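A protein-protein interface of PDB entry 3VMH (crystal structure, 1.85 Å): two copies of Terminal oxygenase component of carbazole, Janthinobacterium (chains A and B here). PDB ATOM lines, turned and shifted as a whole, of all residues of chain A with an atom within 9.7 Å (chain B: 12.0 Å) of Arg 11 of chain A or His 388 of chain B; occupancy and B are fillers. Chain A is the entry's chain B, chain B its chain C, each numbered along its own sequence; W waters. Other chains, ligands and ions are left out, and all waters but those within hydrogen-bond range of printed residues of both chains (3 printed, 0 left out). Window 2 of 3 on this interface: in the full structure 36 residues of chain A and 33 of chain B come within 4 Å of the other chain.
No position is printed for both chains.
Of the 4 pairs that touch across the chains among the printed residues, none has its exchanged pair printed and touching as well.
Water W1 lies within hydrogen-bond range of OD1 of Asn 352 of chain A and O of Leu 385 of chain B.
Water W3 lies within hydrogen-bond range of the backbone carbonyl oxygen of Gly 384 of chain B (2.7 Å), the side-chain hydroxyl of Ser 383 of chain B (2.9 Å), the side-chain carboxylate of Glu 386 of chain B (3.0 Å) and the side-chain amide nitrogen of Asn 352 of chain A (3.1 Å).
Water W2 lies within hydrogen-bond range of ND2 of Asn 352 of chain A (2.8 Å) and O of Ser 383 of chain B (3.1 Å).
A ring nitrogen (NE2) of His 388 of chain B sits close to the guanidinium group (NH2) of Arg 11 of chain A (3.3 Å).
The side-chain carboxylate (OE2) of Glu 386 of chain B is in salt-bridge range of the side-chain amino group (NZ) of Lys 348 of chain A.
The backbone carbonyl oxygen of Ser 383 of chain B lies within hydrogen-bond range of the side-chain amide nitrogen of Asn 352 of chain A (3.5 Å).
Of the 20 printed residues of chain A, 3 touch a printed residue of chain B.
Among the printed residues, 4 pairs touch across the chains.
Among the printed residues, Asp or Glu carboxylates within 4 Å of a Lys or Arg side-chain nitrogen of the other chain: Lys 348 of chain A with Glu 386 of chain B.
His 387 of chain B touches Arg 11 of chain A.
O of Lys 348 of chain A sits at hydrogen-bond distance from ND2 of Asn 352 of chain A, at 3.5 Å.
Of chain B, only His 387 (3.7 Å) and His 388 (3.2 Å) come within 4 Å of Arg 11 of chain A.
Of chain A, only Arg 11 (3.2 Å) comes within 4 Å of His 388 of chain B.
No residue of chain B comes within 4 Å of Ala 7 of chain A.
No residue of chain B comes within 4 Å of Ile 8 of chain A.
No residue of chain B comes within 4 Å of Val 12 of chain A.
Lys 13 of chain A touches none of the printed residues of chain B.
No residue of chain B comes within 4 Å of Val 351 of chain A.
Of chain A, only Arg 11 comes within 4 Å of His 387 of chain B.
Of the printed residues of chain B, Asn 352 of chain A touches Ser 383.
Of the printed residues of chain A, Glu 386 of chain B touches Lys 348 (2.8 Å).
Ala 16 of chain A touches none of the printed residues of chain B.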
ATOM      1  N   VAL A   4      33.967 -16.478 -30.597  1.00  0.00           N
ATOM      2  CA  VAL A   4      32.579 -16.723 -30.224  1.00  0.00           C
ATOM      3  C   VAL A   4      32.283 -16.252 -28.804  1.00  0.00           C
ATOM      4  O   VAL A   4      33.180 -16.186 -27.964  1.00  0.00           O
ATOM      5  CB  VAL A   4      32.267 -18.233 -30.317  1.00  0.00           C
ATOM      6  CG1 VAL A   4      30.829 -18.514 -29.893  1.00  0.00           C
ATOM      7  CG2 VAL A   4      32.523 -18.720 -31.735  1.00  0.00           C
ATOM      8  N   ASP A   5      31.015 -15.931 -28.555  1.00  0.00           N
ATOM      9  CA  ASP A   5      30.554 -15.486 -27.242  1.00  0.00           C
ATOM     10  C   ASP A   5      31.121 -16.426 -26.184  1.00  0.00           C
ATOM     11  O   ASP A   5      30.982 -17.648 -26.287  1.00  0.00           O
ATOM     12  CB  ASP A   5      29.022 -15.520 -27.185  1.00  0.00           C
ATOM     13  CG  ASP A   5      28.468 -14.935 -25.897  1.00  0.00           C
ATOM     14  OD1 ASP A   5      29.076 -15.150 -24.829  1.00  0.00           O
ATOM     15  OD2 ASP A   5      27.413 -14.268 -25.952  1.00  0.00           O
ATOM     16  N   GLU A   6      31.753 -15.854 -25.168  1.00  0.00           N
ATOM     17  CA  GLU A   6      32.353 -16.646 -24.103  1.00  0.00           C
ATOM     18  C   GLU A   6      31.335 -17.526 -23.384  1.00  0.00           C
ATOM     19  O   GLU A   6      31.681 -18.596 -22.889  1.00  0.00           O
ATOM     20  CB  GLU A   6      33.039 -15.727 -23.092  1.00  0.00           C
ATOM     21  CG  GLU A   6      34.173 -16.399 -22.349  1.00  0.00           C
ATOM     22  CD  GLU A   6      35.209 -16.989 -23.295  1.00  0.00           C
ATOM     23  OE1 GLU A   6      35.633 -16.279 -24.234  1.00  0.00           O
ATOM     24  OE2 GLU A   6      35.603 -18.160 -23.096  1.00  0.00           O
ATOM     25  N   ALA A   7      30.087 -17.073 -23.326  1.00  0.00           N
ATOM     26  CA  ALA A   7      29.031 -17.834 -22.660  1.00  0.00           C
ATOM     27  C   ALA A   7      28.774 -19.147 -23.389  1.00  0.00           C
ATOM     28  O   ALA A   7      28.421 -20.151 -22.770  1.00  0.00           O
ATOM     29  CB  ALA A   7      27.742 -17.011 -22.597  1.00  0.00           C
ATOM     30  N   ILE A   8      28.948 -19.138 -24.707  1.00  0.00           N
ATOM     31  CA  ILE A   8      28.736 -20.344 -25.498  1.00  0.00           C
ATOM     32  C   ILE A   8      29.920 -21.290 -25.345  1.00  0.00           C
ATOM     33  O   ILE A   8      29.747 -22.493 -25.170  1.00  0.00           O
ATOM     34  CB  ILE A   8      28.530 -20.003 -26.993  1.00  0.00           C
ATOM     35  CG1 ILE A   8      27.192 -19.279 -27.175  1.00  0.00           C
ATOM     36  CG2 ILE A   8      28.564 -21.275 -27.831  1.00  0.00           C
ATOM     37  CD1 ILE A   8      26.950 -18.756 -28.578  1.00  0.00           C
ATOM     38  N   LEU A   9      31.132 -20.749 -25.404  1.00  0.00           N
ATOM     39  CA  LEU A   9      32.313 -21.588 -25.265  1.00  0.00           C
ATOM     40  C   LEU A   9      32.321 -22.271 -23.902  1.00  0.00           C
ATOM     41  O   LEU A   9      32.771 -23.405 -23.774  1.00  0.00           O
ATOM     42  CB  LEU A   9      33.586 -20.756 -25.448  1.00  0.00           C
ATOM     43  CG  LEU A   9      33.775 -20.137 -26.835  1.00  0.00           C
ATOM     44  CD1 LEU A   9      35.096 -19.375 -26.874  1.00  0.00           C
ATOM     45  CD2 LEU A   9      33.762 -21.236 -27.902  1.00  0.00           C
ATOM     46  N   LYS A  10      31.815 -21.578 -22.887  1.00  0.00           N
ATOM     47  CA  LYS A  10      31.766 -22.135 -21.541  1.00  0.00           C
ATOM     48  C   LYS A  10      30.828 -23.341 -21.490  1.00  0.00           C
ATOM     49  O   LYS A  10      31.031 -24.264 -20.700  1.00  0.00           O
ATOM     50  CB  LYS A  10      31.290 -21.076 -20.544  1.00  0.00           C
ATOM     51  CG  LYS A  10      31.213 -21.584 -19.109  1.00  0.00           C
ATOM     52  CD  LYS A  10      30.813 -20.483 -18.137  1.00  0.00           C
ATOM     53  CE  LYS A  10      30.754 -21.015 -16.710  1.00  0.00           C
ATOM     54  NZ  LYS A  10      29.743 -22.105 -16.563  1.00  0.00           N
ATOM     55  N   ARG A  11      29.804 -23.326 -22.338  1.00  0.00           N
ATOM     56  CA  ARG A  11      28.830 -24.412 -22.386  1.00  0.00           C
ATOM     57  C   ARG A  11      29.332 -25.672 -23.091  1.00  0.00           C
ATOM     58  O   ARG A  11      29.021 -26.782 -22.667  1.00  0.00           O
ATOM     59  CB  ARG A  11      27.540 -23.935 -23.062  1.00  0.00           C
ATOM     60  CG  ARG A  11      26.541 -23.262 -22.123  1.00  0.00           C
ATOM     61  CD  ARG A  11      25.341 -22.736 -22.896  1.00  0.00           C
ATOM     62  NE  ARG A  11      24.249 -22.286 -22.031  1.00  0.00           N
ATOM     63  CZ  ARG A  11      23.388 -23.099 -21.424  1.00  0.00           C
ATOM     64  NH1 ARG A  11      23.483 -24.414 -21.581  1.00  0.00           N
ATOM     65  NH2 ARG A  11      22.422 -22.597 -20.666  1.00  0.00           N
ATOM     66  N   VAL A  12      30.099 -25.508 -24.165  1.00  0.00           N
ATOM     67  CA  VAL A  12      30.609 -26.662 -24.905  1.00  0.00           C
ATOM     68  C   VAL A  12      31.990 -27.084 -24.412  1.00  0.00           C
ATOM     69  O   VAL A  12      32.980 -26.993 -25.134  1.00  0.00           O
ATOM     70  CB  VAL A  12      30.667 -26.365 -26.420  1.00  0.00           C
ATOM     71  CG1 VAL A  12      29.257 -26.205 -26.964  1.00  0.00           C
ATOM     72  CG2 VAL A  12      31.475 -25.096 -26.683  1.00  0.00           C
ATOM     73  N   LYS A  13      32.028 -27.578 -23.176  1.00  0.00           N
ATOM     74  CA  LYS A  13      33.262 -27.998 -22.526  1.00  0.00           C
ATOM     75  C   LYS A  13      34.073 -29.092 -23.213  1.00  0.00           C
ATOM     76  O   LYS A  13      35.279 -29.182 -23.008  1.00  0.00           O
ATOM     77  CB  LYS A  13      32.958 -28.437 -21.092  1.00  0.00           C
ATOM     78  CG  LYS A  13      32.362 -27.339 -20.227  1.00  0.00           C
ATOM     79  CD  LYS A  13      32.129 -27.818 -18.804  1.00  0.00           C
ATOM     80  CE  LYS A  13      31.618 -26.687 -17.923  1.00  0.00           C
ATOM     81  NZ  LYS A  13      30.317 -26.144 -18.416  1.00  0.00           N
ATOM     82  N   GLY A  14      33.424 -29.925 -24.016  1.00  0.00           N
ATOM     83  CA  GLY A  14      34.145 -30.998 -24.678  1.00  0.00           C
ATOM     84  C   GLY A  14      34.880 -30.624 -25.955  1.00  0.00           C
ATOM     85  O   GLY A  14      35.750 -31.372 -26.407  1.00  0.00           O
ATOM     86  N   TRP A  15      34.547 -29.477 -26.541  1.00  0.00           N
ATOM     87  CA  TRP A  15      35.191 -29.064 -27.785  1.00  0.00           C
ATOM     88  C   TRP A  15      35.127 -27.559 -28.069  1.00  0.00           C
ATOM     89  O   TRP A  15      34.838 -27.137 -29.191  1.00  0.00           O
ATOM     90  CB  TRP A  15      34.583 -29.865 -28.950  1.00  0.00           C
ATOM     91  CG  TRP A  15      33.068 -29.878 -28.990  1.00  0.00           C
ATOM     92  CD1 TRP A  15      32.254 -28.899 -29.473  1.00  0.00           C
ATOM     93  CD2 TRP A  15      32.201 -30.928 -28.527  1.00  0.00           C
ATOM     94  NE1 TRP A  15      30.931 -29.269 -29.344  1.00  0.00           N
ATOM     95  CE2 TRP A  15      30.871 -30.508 -28.766  1.00  0.00           C
ATOM     96  CE3 TRP A  15      32.418 -32.181 -27.936  1.00  0.00           C
ATOM     97  CZ2 TRP A  15      29.758 -31.298 -28.432  1.00  0.00           C
ATOM     98  CZ3 TRP A  15      31.310 -32.968 -27.602  1.00  0.00           C
ATOM     99  CH2 TRP A  15      29.997 -32.520 -27.852  1.00  0.00           C
ATOM    100  N   ALA A  16      35.429 -26.754 -27.053  1.00  0.00           N
ATOM    101  CA  ALA A  16      35.393 -25.299 -27.191  1.00  0.00           C
ATOM    102  C   ALA A  16      36.359 -24.741 -28.238  1.00  0.00           C
ATOM    103  O   ALA A  16      36.027 -23.804 -28.962  1.00  0.00           O
ATOM    104  CB  ALA A  16      35.654 -24.641 -25.839  1.00  0.00           C
ATOM    105  N   VAL A  19      34.697 -25.038 -31.609  1.00  0.00           N
ATOM    106  CA  VAL A  19      33.595 -24.105 -31.775  1.00  0.00           C
ATOM    107  C   VAL A  19      34.141 -22.695 -32.001  1.00  0.00           C
ATOM    108  O   VAL A  19      33.555 -21.901 -32.726  1.00  0.00           O
ATOM    109  CB  VAL A  19      32.674 -24.120 -30.532  1.00  0.00           C
ATOM    110  CG1 VAL A  19      31.659 -22.984 -30.605  1.00  0.00           C
ATOM    111  CG2 VAL A  19      31.955 -25.463 -30.447  1.00  0.00           C
ATOM    112  N   ASP A 347      25.960 -19.139 -33.805  1.00  0.00           N
ATOM    113  CA  ASP A 347      26.732 -19.959 -32.865  1.00  0.00           C
ATOM    114  C   ASP A 347      25.846 -20.738 -31.875  1.00  0.00           C
ATOM    115  O   ASP A 347      26.317 -21.532 -31.072  1.00  0.00           O
ATOM    116  CB  ASP A 347      27.681 -19.035 -32.099  1.00  0.00           C
ATOM    117  CG  ASP A 347      28.796 -18.578 -33.027  1.00  0.00           C
ATOM    118  OD1 ASP A 347      29.234 -19.393 -33.841  1.00  0.00           O
ATOM    119  OD2 ASP A 347      29.209 -17.425 -32.933  1.00  0.00           O
ATOM    120  N   LYS A 348      24.537 -20.517 -31.918  1.00  0.00           N
ATOM    121  CA  LYS A 348      23.618 -21.181 -30.991  1.00  0.00           C
ATOM    122  C   LYS A 348      23.416 -22.662 -31.305  1.00  0.00           C
ATOM    123  O   LYS A 348      23.162 -23.466 -30.409  1.00  0.00           O
ATOM    124  CB  LYS A 348      22.262 -20.476 -30.996  1.00  0.00           C
ATOM    125  CG  LYS A 348      22.325 -18.983 -30.726  1.00  0.00           C
ATOM    126  CD  LYS A 348      22.498 -18.662 -29.262  1.00  0.00           C
ATOM    127  CE  LYS A 348      22.343 -17.158 -29.035  1.00  0.00           C
ATOM    128  NZ  LYS A 348      22.161 -16.812 -27.601  1.00  0.00           N
ATOM    129  N   TRP A 350      25.472 -24.830 -31.860  1.00  0.00           N
ATOM    130  CA  TRP A 350      26.473 -25.625 -31.148  1.00  0.00           C
ATOM    131  C   TRP A 350      25.999 -26.006 -29.744  1.00  0.00           C
ATOM    132  O   TRP A 350      26.607 -26.853 -29.076  1.00  0.00           O
ATOM    133  CB  TRP A 350      27.795 -24.853 -31.046  1.00  0.00           C
ATOM    134  CG  TRP A 350      28.398 -24.508 -32.374  1.00  0.00           C
ATOM    135  CD1 TRP A 350      28.530 -23.260 -32.917  1.00  0.00           C
ATOM    136  CD2 TRP A 350      28.931 -25.422 -33.334  1.00  0.00           C
ATOM    137  NE1 TRP A 350      29.115 -23.342 -34.160  1.00  0.00           N
ATOM    138  CE2 TRP A 350      29.369 -24.659 -34.442  1.00  0.00           C
ATOM    139  CE3 TRP A 350      29.082 -26.818 -33.369  1.00  0.00           C
ATOM    140  CZ2 TRP A 350      29.946 -25.243 -35.574  1.00  0.00           C
ATOM    141  CZ3 TRP A 350      29.654 -27.399 -34.494  1.00  0.00           C
ATOM    142  CH2 TRP A 350      30.080 -26.611 -35.584  1.00  0.00           C
ATOM    143  N   VAL A 351      24.921 -25.369 -29.297  1.00  0.00           N
ATOM    144  CA  VAL A 351      24.360 -25.649 -27.981  1.00  0.00           C
ATOM    145  C   VAL A 351      23.015 -26.363 -28.082  1.00  0.00           C
ATOM    146  O   VAL A 351      22.740 -27.292 -27.323  1.00  0.00           O
ATOM    147  CB  VAL A 351      24.143 -24.346 -27.164  1.00  0.00           C
ATOM    148  CG1 VAL A 351      23.399 -24.657 -25.863  1.00  0.00           C
ATOM    149  CG2 VAL A 351      25.487 -23.694 -26.850  1.00  0.00           C
ATOM    150  N   ASN A 352      22.192 -25.939 -29.038  1.00  0.00           N
ATOM    151  CA  ASN A 352      20.851 -26.498 -29.197  1.00  0.00           C
ATOM    152  C   ASN A 352      20.662 -27.767 -30.034  1.00  0.00           C
ATOM    153  O   ASN A 352      19.582 -28.362 -30.016  1.00  0.00           O
ATOM    154  CB  ASN A 352      19.913 -25.404 -29.710  1.00  0.00           C
ATOM    155  CG  ASN A 352      19.783 -24.255 -28.734  1.00  0.00           C
ATOM    156  OD1 ASN A 352      19.565 -24.468 -27.543  1.00  0.00           O
ATOM    157  ND2 ASN A 352      19.913 -23.032 -29.230  1.00  0.00           N
ATOM    158  N   GLU A 353      21.692 -28.176 -30.766  1.00  0.00           N
ATOM    159  CA  GLU A 353      21.623 -29.388 -31.585  1.00  0.00           C
ATOM    160  C   GLU A 353      21.234 -30.589 -30.709  1.00  0.00           C
ATOM    161  O   GLU A 353      21.694 -30.708 -29.574  1.00  0.00           O
ATOM    162  CB  GLU A 353      22.997 -29.661 -32.204  1.00  0.00           C
ATOM    163  CG  GLU A 353      24.076 -29.833 -31.138  1.00  0.00           C
ATOM    164  CD  GLU A 353      25.484 -29.967 -31.694  1.00  0.00           C
ATOM    165  OE1 GLU A 353      25.684 -29.773 -32.907  1.00  0.00           O
ATOM    166  OE2 GLU A 353      26.397 -30.262 -30.898  1.00  0.00           O
ATOM    167  N   ALA B 380      15.184 -15.352 -28.546  1.00  0.00           N
ATOM    168  CA  ALA B 380      15.449 -16.619 -27.886  1.00  0.00           C
ATOM    169  C   ALA B 380      14.339 -17.610 -28.217  1.00  0.00           C
ATOM    170  O   ALA B 380      14.578 -18.820 -28.282  1.00  0.00           O
ATOM    171  CB  ALA B 380      15.556 -16.420 -26.374  1.00  0.00           C
ATOM    172  N   SER B 383      15.548 -18.965 -31.611  1.00  0.00           N
ATOM    173  CA  SER B 383      16.688 -19.883 -31.616  1.00  0.00           C
ATOM    174  C   SER B 383      16.545 -21.036 -30.626  1.00  0.00           C
ATOM    175  O   SER B 383      16.996 -22.149 -30.892  1.00  0.00           O
ATOM    176  CB  SER B 383      17.986 -19.117 -31.333  1.00  0.00           C
ATOM    177  OG  SER B 383      17.949 -18.509 -30.053  1.00  0.00           O
ATOM    178  N   GLY B 384      15.912 -20.760 -29.492  1.00  0.00           N
ATOM    179  CA  GLY B 384      15.720 -21.771 -28.467  1.00  0.00           C
ATOM    180  C   GLY B 384      15.810 -21.089 -27.118  1.00  0.00           C
ATOM    181  O   GLY B 384      16.835 -20.484 -26.809  1.00  0.00           O
ATOM    182  N   LEU B 385      14.750 -21.174 -26.319  1.00  0.00           N
ATOM    183  CA  LEU B 385      14.742 -20.521 -25.013  1.00  0.00           C
ATOM    184  C   LEU B 385      15.948 -20.914 -24.174  1.00  0.00           C
ATOM    185  O   LEU B 385      16.384 -22.069 -24.182  1.00  0.00           O
ATOM    186  CB  LEU B 385      13.444 -20.826 -24.261  1.00  0.00           C
ATOM    187  CG  LEU B 385      12.197 -20.126 -24.817  1.00  0.00           C
ATOM    188  CD1 LEU B 385      10.981 -20.548 -24.019  1.00  0.00           C
ATOM    189  CD2 LEU B 385      12.376 -18.607 -24.756  1.00  0.00           C
ATOM    190  N   GLU B 386      16.481 -19.938 -23.450  1.00  0.00           N
ATOM    191  CA  GLU B 386      17.661 -20.147 -22.630  1.00  0.00           C
ATOM    192  C   GLU B 386      17.385 -19.874 -21.157  1.00  0.00           C
ATOM    193  O   GLU B 386      16.637 -18.959 -20.808  1.00  0.00           O
ATOM    194  CB  GLU B 386      18.783 -19.241 -23.140  1.00  0.00           C
ATOM    195  CG  GLU B 386      18.895 -19.246 -24.665  1.00  0.00           C
ATOM    196  CD  GLU B 386      19.907 -18.251 -25.200  1.00  0.00           C
ATOM    197  OE1 GLU B 386      19.944 -17.106 -24.698  1.00  0.00           O
ATOM    198  OE2 GLU B 386      20.654 -18.610 -26.136  1.00  0.00           O
ATOM    199  N   HIS B 387      17.991 -20.686 -20.298  1.00  0.00           N
ATOM    200  CA  HIS B 387      17.835 -20.551 -18.857  1.00  0.00           C
ATOM    201  C   HIS B 387      19.014 -21.236 -18.178  1.00  0.00           C
ATOM    202  O   HIS B 387      19.363 -22.367 -18.515  1.00  0.00           O
ATOM    203  CB  HIS B 387      16.541 -21.217 -18.387  1.00  0.00           C
ATOM    204  CG  HIS B 387      16.264 -21.030 -16.926  1.00  0.00           C
ATOM    205  ND1 HIS B 387      15.678 -22.006 -16.149  1.00  0.00           N
ATOM    206  CD2 HIS B 387      16.475 -19.971 -16.107  1.00  0.00           C
ATOM    207  CE1 HIS B 387      15.539 -21.557 -14.913  1.00  0.00           C
ATOM    208  NE2 HIS B 387      16.013 -20.325 -14.861  1.00  0.00           N
ATOM    209  N   HIS B 388      19.623 -20.545 -17.221  1.00  0.00           N
ATOM    210  CA  HIS B 388      20.759 -21.098 -16.496  1.00  0.00           C
ATOM    211  C   HIS B 388      20.379 -21.370 -15.046  1.00  0.00           C
ATOM    212  O   HIS B 388      19.846 -20.494 -14.362  1.00  0.00           O
ATOM    213  CB  HIS B 388      21.944 -20.126 -16.548  1.00  0.00           C
ATOM    214  CG  HIS B 388      22.516 -19.939 -17.920  1.00  0.00           C
ATOM    215  ND1 HIS B 388      21.739 -19.622 -19.016  1.00  0.00           N
ATOM    216  CD2 HIS B 388      23.792 -20.007 -18.372  1.00  0.00           C
ATOM    217  CE1 HIS B 388      22.512 -19.503 -20.081  1.00  0.00           C
ATOM    218  NE2 HIS B 388      23.762 -19.731 -19.718  1.00  0.00           N
ATOM    219  N   HIS B 389      20.647 -22.593 -14.592  1.00  0.00           N
ATOM    220  CA  HIS B 389      20.353 -22.999 -13.220  1.00  0.00           C
ATOM    221  C   HIS B 389      20.761 -21.899 -12.245  1.00  0.00           C
ATOM    222  O   HIS B 389      21.940 -21.550 -12.148  1.00  0.00           O
ATOM    223  CB  HIS B 389      21.112 -24.281 -12.872  1.00  0.00           C
ATOM    224  CG  HIS B 389      21.070 -24.625 -11.416  1.00  0.00           C
ATOM    225  ND1 HIS B 389      22.153 -25.151 -10.746  1.00  0.00           N
ATOM    226  CD2 HIS B 389      20.079 -24.511 -10.500  1.00  0.00           C
ATOM    227  CE1 HIS B 389      21.832 -25.343  -9.478  1.00  0.00           C
ATOM    228  NE2 HIS B 389      20.579 -24.963  -9.302  1.00  0.00           N
ATOM    229  N   HIS B 390      19.785 -21.367 -11.515  1.00  0.00           N
ATOM    230  CA  HIS B 390      20.042 -20.299 -10.558  1.00  0.00           C
ATOM    231  C   HIS B 390      20.593 -20.845  -9.241  1.00  0.00           C
ATOM    232  O   HIS B 390      20.680 -22.083  -9.096  1.00  0.00           O
ATOM    233  CB  HIS B 390      18.752 -19.518 -10.298  1.00  0.00           C
ATOM    234  CG  HIS B 390      18.970 -18.185  -9.656  1.00  0.00           C
ATOM    235  ND1 HIS B 390      19.580 -17.137 -10.312  1.00  0.00           N
ATOM    236  CD2 HIS B 390      18.676 -17.733  -8.414  1.00  0.00           C
ATOM    237  CE1 HIS B 390      19.652 -16.096  -9.500  1.00  0.00           C
ATOM    238  NE2 HIS B 390      19.111 -16.431  -8.342  1.00  0.00           N
HETATM  239  O   HOH W   1      18.798 -23.224 -25.359  1.00  0.00           O
HETATM  240  O   HOH W   2      19.865 -22.477 -32.005  1.00  0.00           O
HETATM  241  O   HOH W   3      19.129 -20.266 -28.128  1.00  0.00           O
